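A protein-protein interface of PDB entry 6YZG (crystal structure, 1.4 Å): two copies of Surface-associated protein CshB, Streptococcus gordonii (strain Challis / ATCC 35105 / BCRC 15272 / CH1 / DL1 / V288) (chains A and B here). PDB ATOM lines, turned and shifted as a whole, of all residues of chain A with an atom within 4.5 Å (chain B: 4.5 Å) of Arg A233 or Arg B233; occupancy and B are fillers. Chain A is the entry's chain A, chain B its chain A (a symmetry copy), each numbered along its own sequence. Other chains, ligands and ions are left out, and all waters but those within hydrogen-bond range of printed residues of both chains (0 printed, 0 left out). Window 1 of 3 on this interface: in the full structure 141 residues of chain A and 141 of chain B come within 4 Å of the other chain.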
ATOM      1  N   ASP A 147      27.750 -24.111  11.090  1.00  0.00           N
ATOM      2  CA  ASP A 147      27.294 -23.183  10.037  1.00  0.00           C
ATOM      3  C   ASP A 147      27.792 -23.702   8.682  1.00  0.00           C
ATOM      4  O   ASP A 147      28.769 -24.397   8.617  1.00  0.00           O
ATOM      5  CB  ASP A 147      27.820 -21.763  10.253  1.00  0.00           C
ATOM      6  CG  ASP A 147      26.791 -20.711   9.840  1.00  0.00           C
ATOM      7  OD1 ASP A 147      25.876 -21.036   9.097  1.00  0.00           O
ATOM      8  OD2 ASP A 147      26.859 -19.592  10.336  1.00  0.00           O
ATOM      9  N   TRP A 169      16.953 -24.608  16.197  1.00  0.00           N
ATOM     10  CA  TRP A 169      17.678 -24.845  17.452  1.00  0.00           C
ATOM     11  C   TRP A 169      18.752 -23.755  17.598  1.00  0.00           C
ATOM     12  O   TRP A 169      19.537 -23.559  16.683  1.00  0.00           O
ATOM     13  CB  TRP A 169      18.270 -26.252  17.472  1.00  0.00           C
ATOM     14  CG  TRP A 169      18.939 -26.592  18.762  1.00  0.00           C
ATOM     15  CD1 TRP A 169      20.272 -26.507  19.042  1.00  0.00           C
ATOM     16  CD2 TRP A 169      18.304 -27.089  19.943  1.00  0.00           C
ATOM     17  NE1 TRP A 169      20.516 -26.940  20.325  1.00  0.00           N
ATOM     18  CE2 TRP A 169      19.323 -27.275  20.909  1.00  0.00           C
ATOM     19  CE3 TRP A 169      16.986 -27.447  20.251  1.00  0.00           C
ATOM     20  CZ2 TRP A 169      19.043 -27.781  22.173  1.00  0.00           C
ATOM     21  CZ3 TRP A 169      16.712 -27.934  21.512  1.00  0.00           C
ATOM     22  CH2 TRP A 169      17.729 -28.080  22.454  1.00  0.00           C
ATOM     23  N   LYS A 170      18.692 -23.070  18.732  1.00  0.00           N
ATOM     24  CA  LYS A 170      19.547 -21.894  19.033  1.00  0.00           C
ATOM     25  C   LYS A 170      20.902 -22.342  19.561  1.00  0.00           C
ATOM     26  O   LYS A 170      20.923 -23.105  20.528  1.00  0.00           O
ATOM     27  CB  LYS A 170      18.827 -20.965  20.017  1.00  0.00           C
ATOM     28  CG  LYS A 170      19.662 -19.835  20.595  1.00  0.00           C
ATOM     29  CD  LYS A 170      20.146 -18.869  19.554  1.00  0.00           C
ATOM     30  CE  LYS A 170      19.332 -17.594  19.498  1.00  0.00           C
ATOM     31  NZ  LYS A 170      19.654 -16.781  18.301  1.00  0.00           N
ATOM     32  N   MET A 171      21.948 -21.853  18.894  1.00  0.00           N
ATOM     33  CA  MET A 171      23.371 -22.117  19.222  1.00  0.00           C
ATOM     34  C   MET A 171      23.990 -20.836  19.798  1.00  0.00           C
ATOM     35  O   MET A 171      23.562 -20.433  20.861  1.00  0.00           O
ATOM     36  CB  MET A 171      24.131 -22.513  17.959  1.00  0.00           C
ATOM     37  CG  MET A 171      23.672 -23.824  17.379  1.00  0.00           C
ATOM     38  SD  MET A 171      24.032 -25.232  18.433  1.00  0.00           S
ATOM     39  CE  MET A 171      24.534 -26.382  17.166  1.00  0.00           C
ATOM     40  N   SER A 230      21.402 -21.801   7.182  1.00  0.00           N
ATOM     41  CA  SER A 230      20.508 -20.982   8.049  1.00  0.00           C
ATOM     42  C   SER A 230      20.533 -19.549   7.503  1.00  0.00           C
ATOM     43  O   SER A 230      21.614 -19.196   6.983  1.00  0.00           O
ATOM     44  CB  SER A 230      20.914 -21.011   9.512  1.00  0.00           C
ATOM     45  OG  SER A 230      20.231 -19.975  10.214  1.00  0.00           O
ATOM     46  N   ASN A 231      19.377 -18.852   7.545  1.00  0.00           N
ATOM     47  CA  ASN A 231      19.105 -17.575   6.822  1.00  0.00           C
ATOM     48  C   ASN A 231      18.882 -16.417   7.812  1.00  0.00           C
ATOM     49  O   ASN A 231      18.668 -15.275   7.335  1.00  0.00           O
ATOM     50  CB  ASN A 231      17.931 -17.717   5.826  1.00  0.00           C
ATOM     51  CG  ASN A 231      16.540 -17.662   6.430  1.00  0.00           C
ATOM     52  OD1 ASN A 231      16.378 -17.725   7.642  1.00  0.00           O
ATOM     53  ND2 ASN A 231      15.512 -17.596   5.590  1.00  0.00           N
ATOM     54  N   GLU A 232      18.904 -16.667   9.124  1.00  0.00           N
ATOM     55  CA  GLU A 232      18.634 -15.584  10.102  1.00  0.00           C
ATOM     56  C   GLU A 232      19.949 -15.207  10.785  1.00  0.00           C
ATOM     57  O   GLU A 232      20.491 -16.034  11.546  1.00  0.00           O
ATOM     58  CB  GLU A 232      17.500 -15.928  11.071  1.00  0.00           C
ATOM     59  CG  GLU A 232      17.705 -17.168  11.921  1.00  0.00           C
ATOM     60  CD  GLU A 232      16.584 -17.318  12.936  1.00  0.00           C
ATOM     61  OE1 GLU A 232      16.880 -17.577  14.124  1.00  0.00           O
ATOM     62  OE2 GLU A 232      15.412 -17.144  12.535  1.00  0.00           O
ATOM     63  N   ARG A 233      20.439 -14.002  10.483  1.00  0.00           N
ATOM     64  CA  ARG A 233      21.602 -13.384  11.160  1.00  0.00           C
ATOM     65  C   ARG A 233      21.185 -12.049  11.793  1.00  0.00           C
ATOM     66  O   ARG A 233      20.156 -11.416  11.343  1.00  0.00           O
ATOM     67  CB  ARG A 233      22.767 -13.162  10.193  1.00  0.00           C
ATOM     68  CG  ARG A 233      23.959 -14.080  10.430  1.00  0.00           C
ATOM     69  CD  ARG A 233      24.592 -14.092  11.828  1.00  0.00           C
ATOM     70  NE  ARG A 233      25.663 -15.095  11.845  1.00  0.00           N
ATOM     71  CZ  ARG A 233      26.357 -15.518  12.911  1.00  0.00           C
ATOM     72  NH1 ARG A 233      27.297 -16.438  12.753  1.00  0.00           N
ATOM     73  NH2 ARG A 233      26.116 -15.052  14.126  1.00  0.00           N
ATOM     74  N   THR A 234      21.974 -11.637  12.786  1.00  0.00           N
ATOM     75  CA  THR A 234      21.829 -10.292  13.371  1.00  0.00           C
ATOM     76  C   THR A 234      23.179  -9.609  13.359  1.00  0.00           C
ATOM     77  O   THR A 234      24.226 -10.238  13.240  1.00  0.00           O
ATOM     78  CB  THR A 234      21.204 -10.288  14.769  1.00  0.00           C
ATOM     79  OG1 THR A 234      22.154 -10.831  15.677  1.00  0.00           O
ATOM     80  CG2 THR A 234      19.872 -11.008  14.798  1.00  0.00           C
ATOM     81  N   ASP B 147      28.010 -10.179   7.353  1.00  0.00           N
ATOM     82  CA  ASP B 147      28.594 -11.133   8.315  1.00  0.00           C
ATOM     83  C   ASP B 147      30.122 -11.039   8.228  1.00  0.00           C
ATOM     84  O   ASP B 147      30.653 -10.660   7.220  1.00  0.00           O
ATOM     85  CB  ASP B 147      28.164 -12.573   8.031  1.00  0.00           C
ATOM     86  CG  ASP B 147      27.960 -13.367   9.321  1.00  0.00           C
ATOM     87  OD1 ASP B 147      28.465 -12.956  10.355  1.00  0.00           O
ATOM     88  OD2 ASP B 147      27.222 -14.346   9.301  1.00  0.00           O
ATOM     89  N   TRP B 169      20.322  -5.809  15.396  1.00  0.00           N
ATOM     90  CA  TRP B 169      19.445  -5.540  14.250  1.00  0.00           C
ATOM     91  C   TRP B 169      19.328  -6.830  13.423  1.00  0.00           C
ATOM     92  O   TRP B 169      20.342  -7.403  13.058  1.00  0.00           O
ATOM     93  CB  TRP B 169      19.978  -4.368  13.429  1.00  0.00           C
ATOM     94  CG  TRP B 169      19.081  -3.980  12.302  1.00  0.00           C
ATOM     95  CD1 TRP B 169      19.187  -4.368  10.998  1.00  0.00           C
ATOM     96  CD2 TRP B 169      17.947  -3.114  12.380  1.00  0.00           C
ATOM     97  NE1 TRP B 169      18.198  -3.778  10.246  1.00  0.00           N
ATOM     98  CE2 TRP B 169      17.406  -3.028  11.073  1.00  0.00           C
ATOM     99  CE3 TRP B 169      17.378  -2.360  13.414  1.00  0.00           C
ATOM    100  CZ2 TRP B 169      16.301  -2.231  10.794  1.00  0.00           C
ATOM    101  CZ3 TRP B 169      16.272  -1.584  13.135  1.00  0.00           C
ATOM    102  CH2 TRP B 169      15.742  -1.540  11.846  1.00  0.00           C
ATOM    103  N   LYS B 170      18.084  -7.243  13.217  1.00  0.00           N
ATOM    104  CA  LYS B 170      17.739  -8.525  12.554  1.00  0.00           C
ATOM    105  C   LYS B 170      17.768  -8.367  11.041  1.00  0.00           C
ATOM    106  O   LYS B 170      17.093  -7.467  10.539  1.00  0.00           O
ATOM    107  CB  LYS B 170      16.375  -9.017  13.052  1.00  0.00           C
ATOM    108  CG  LYS B 170      15.781 -10.198  12.302  1.00  0.00           C
ATOM    109  CD  LYS B 170      16.616 -11.441  12.405  1.00  0.00           C
ATOM    110  CE  LYS B 170      16.086 -12.434  13.417  1.00  0.00           C
ATOM    111  NZ  LYS B 170      17.059 -13.518  13.693  1.00  0.00           N
ATOM    112  N   MET B 171      18.552  -9.240  10.406  1.00  0.00           N
ATOM    113  CA  MET B 171      18.735  -9.312   8.935  1.00  0.00           C
ATOM    114  C   MET B 171      18.040 -10.577   8.413  1.00  0.00           C
ATOM    115  O   MET B 171      16.830 -10.637   8.515  1.00  0.00           O
ATOM    116  CB  MET B 171      20.222  -9.387   8.599  1.00  0.00           C
ATOM    117  CG  MET B 171      20.976  -8.137   8.970  1.00  0.00           C
ATOM    118  SD  MET B 171      20.493  -6.703   8.003  1.00  0.00           S
ATOM    119  CE  MET B 171      22.113  -5.998   7.760  1.00  0.00           C
ATOM    120  N   SER B 230      29.131 -11.393  14.981  1.00  0.00           N
ATOM    121  CA  SER B 230      27.853 -11.758  15.657  1.00  0.00           C
ATOM    122  C   SER B 230      27.975 -13.221  16.100  1.00  0.00           C
ATOM    123  O   SER B 230      28.671 -13.946  15.356  1.00  0.00           O
ATOM    124  CB  SER B 230      26.637 -11.559  14.772  1.00  0.00           C
ATOM    125  OG  SER B 230      25.513 -12.216  15.354  1.00  0.00           O
ATOM    126  N   ASN B 231      27.412 -13.558  17.280  1.00  0.00           N
ATOM    127  CA  ASN B 231      27.651 -14.828  18.026  1.00  0.00           C
ATOM    128  C   ASN B 231      26.365 -15.670  18.110  1.00  0.00           C
ATOM    129  O   ASN B 231      26.432 -16.781  18.692  1.00  0.00           O
ATOM    130  CB  ASN B 231      28.264 -14.568  19.422  1.00  0.00           C
ATOM    131  CG  ASN B 231      27.291 -14.128  20.500  1.00  0.00           C
ATOM    132  OD1 ASN B 231      26.148 -13.791  20.216  1.00  0.00           O
ATOM    133  ND2 ASN B 231      27.745 -14.074  21.748  1.00  0.00           N
ATOM    134  N   GLU B 232      25.235 -15.187  17.587  1.00  0.00           N
ATOM    135  CA  GLU B 232      23.966 -15.949  17.704  1.00  0.00           C
ATOM    136  C   GLU B 232      23.619 -16.529  16.332  1.00  0.00           C
ATOM    137  O   GLU B 232      23.301 -15.748  15.411  1.00  0.00           O
ATOM    138  CB  GLU B 232      22.840 -15.131  18.342  1.00  0.00           C
ATOM    139  CG  GLU B 232      22.455 -13.853  17.621  1.00  0.00           C
ATOM    140  CD  GLU B 232      21.238 -13.214  18.269  1.00  0.00           C
ATOM    141  OE1 GLU B 232      20.304 -12.820  17.536  1.00  0.00           O
ATOM    142  OE2 GLU B 232      21.218 -13.138  19.518  1.00  0.00           O
ATOM    143  N   ARG B 233      23.713 -17.855  16.219  1.00  0.00           N
ATOM    144  CA  ARG B 233      23.261 -18.623  15.036  1.00  0.00           C
ATOM    145  C   ARG B 233      22.199 -19.647  15.455  1.00  0.00           C
ATOM    146  O   ARG B 233      22.141 -20.053  16.678  1.00  0.00           O
ATOM    147  CB  ARG B 233      24.428 -19.332  14.344  1.00  0.00           C
ATOM    148  CG  ARG B 233      24.804 -18.744  12.991  1.00  0.00           C
ATOM    149  CD  ARG B 233      23.708 -18.634  11.922  1.00  0.00           C
ATOM    150  NE  ARG B 233      24.274 -17.974  10.741  1.00  0.00           N
ATOM    151  CZ  ARG B 233      23.611 -17.558   9.652  1.00  0.00           C
ATOM    152  NH1 ARG B 233      24.278 -16.975   8.667  1.00  0.00           N
ATOM    153  NH2 ARG B 233      22.300 -17.699   9.542  1.00  0.00           N
ATOM    154  N   THR B 234      21.405 -20.058  14.466  1.00  0.00           N
ATOM    155  CA  THR B 234      20.462 -21.175  14.654  1.00  0.00           C
ATOM    156  C   THR B 234      20.680 -22.187  13.550  1.00  0.00           C
ATOM    157  O   THR B 234      21.263 -21.900  12.510  1.00  0.00           O
ATOM    158  CB  THR B 234      18.996 -20.742  14.744  1.00  0.00           C
ATOM    159  OG1 THR B 234      18.585 -20.312  13.453  1.00  0.00           O
ATOM    160  CG2 THR B 234      18.778 -19.697  15.818  1.00  0.00           C
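OD2 of Asp A147 lies within salt-bridge range of NH1 of Arg A233 (3.998 Å).
The guanidinium group of Arg B233 lies within salt-bridge range of the side-chain carboxylate of Asp B147 (3.998 Å).
Of the 9 printed residues of chain A, 9 touch a printed residue of chain B.
Printed residues of chain A that touch a printed residue of chain B: Asp A147, Trp A169, Lys A170, Met A171, Ser A230, Asn A231, Glu A232, Arg A233 and Thr A234.
Hydrophobic or aromatic side chains of chain A that line the printed part of chain B: Met A171.
Of the 9 printed residues of chain B, 9 touch a printed residue of chain A.
Hydrophobic or aromatic side chains of chain B that line the printed part of chain A: Met B171.
Among the printed residues, 23 pairs touch across the chains.
Among the printed residues, pairs that only touch across the chains: Trp A169 with Thr B234, Lys A170 with Glu B232, Lys A170 with Arg B233, Lys A170 with Thr B234, Asn A231 with Arg B233, Glu A232 with Lys B170, Arg A233 with Lys B170, Arg A233 with Asn B231, Thr A234 with Trp B169 and Thr A234 with Lys B170.
Printed residues of chain B within 4 Å of Arg A233: Asp B147, Lys B170, Met B171, Ser B230, Asn B231, Glu B232 and Arg B233.
Arg B233 touches just these residues of chain A: Asp A147, Lys A170, Met A171, Ser A230, Asn A231, Glu A232 and Arg A233.
Printed residues of chain A within 4 Å of Asp B147: Arg A233.
Printed residues of chain B within 4 Å of Trp A169: Thr B234 (3.3 Å).
Of the printed residues of chain A, Asn B231 touches Arg A233 (3.7 Å).
Of the printed residues of chain B, Asn A231 touches Arg B233 (3.7 Å).
Of the printed residues of chain B, Glu A232 touches Lys B170 (3.6 Å), Arg B233 (3.2 Å) and Thr B234 (3.3 Å).
The nearest residue of chain B that does not touch Arg A233 is Trp B169 (4.4 Å).
The nearest printed residue of chain A that does not touch Trp B169 is Arg A233 (4.4 Å).
Trp A169 touches Thr B234, and with the chains exchanged Thr A234 touches Trp B169.
Lys A170 touches Thr B234, and with the chains exchanged Thr A234 touches Lys B170.
Ser A230 touches Thr B234, and with the chains exchanged Thr A234 touches Ser B230.
Asn A231 touches Arg B233, and with the chains exchanged Arg A233 touches Asn B231.
Of the 23 pairs that touch across the chains among the printed residues, 23 have their exchanged pair printed and touching as well.
The guanidinium group (NE) of Arg A233 sits close to the guanidinium group (NE) of Arg B233.
The backbone NH (N) of Met A171 is in hydrogen-bond range of the backbone carbonyl oxygen (O) of Arg B233 (2.9 Å).
NH2 of Arg B233 is in hydrogen-bond range of O of Glu A232 (3.2 Å).
The side-chain hydroxyl of Ser A230 lies close to the backbone carbonyl oxygen of Thr B234.
NE of Arg A233 is in salt-bridge range of OD2 of Asp B147, 3.1 Å away.
The guanidinium group (NE) of Arg B233 lies within salt-bridge range of the side-chain carboxylate (OD2) of Asp A147, at 3.1 Å.
The backbone NH (N) of Met B171 is in hydrogen-bond range of the backbone carbonyl oxygen (O) of Arg A233.
NH2 of Arg A233 lies within hydrogen-bond range of O of Glu B232, at 3.2 Å.
NH2 of Arg A233 sits at hydrogen-bond distance from O of Ser B230 (3.0 Å).
NH2 of Arg B233 is in hydrogen-bond range of O of Ser A230 (3.0 Å).
The side-chain hydroxyl (OG) of Ser B230 lies close to the backbone carbonyl oxygen (O) of Thr A234.
The side-chain hydroxyl of Thr A234 sits at hydrogen-bond distance from the side-chain carboxylate of Glu B232 (3.3 Å).
OE1 of Glu A232 sits at hydrogen-bond distance from OG1 of Thr B234 (3.3 Å).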
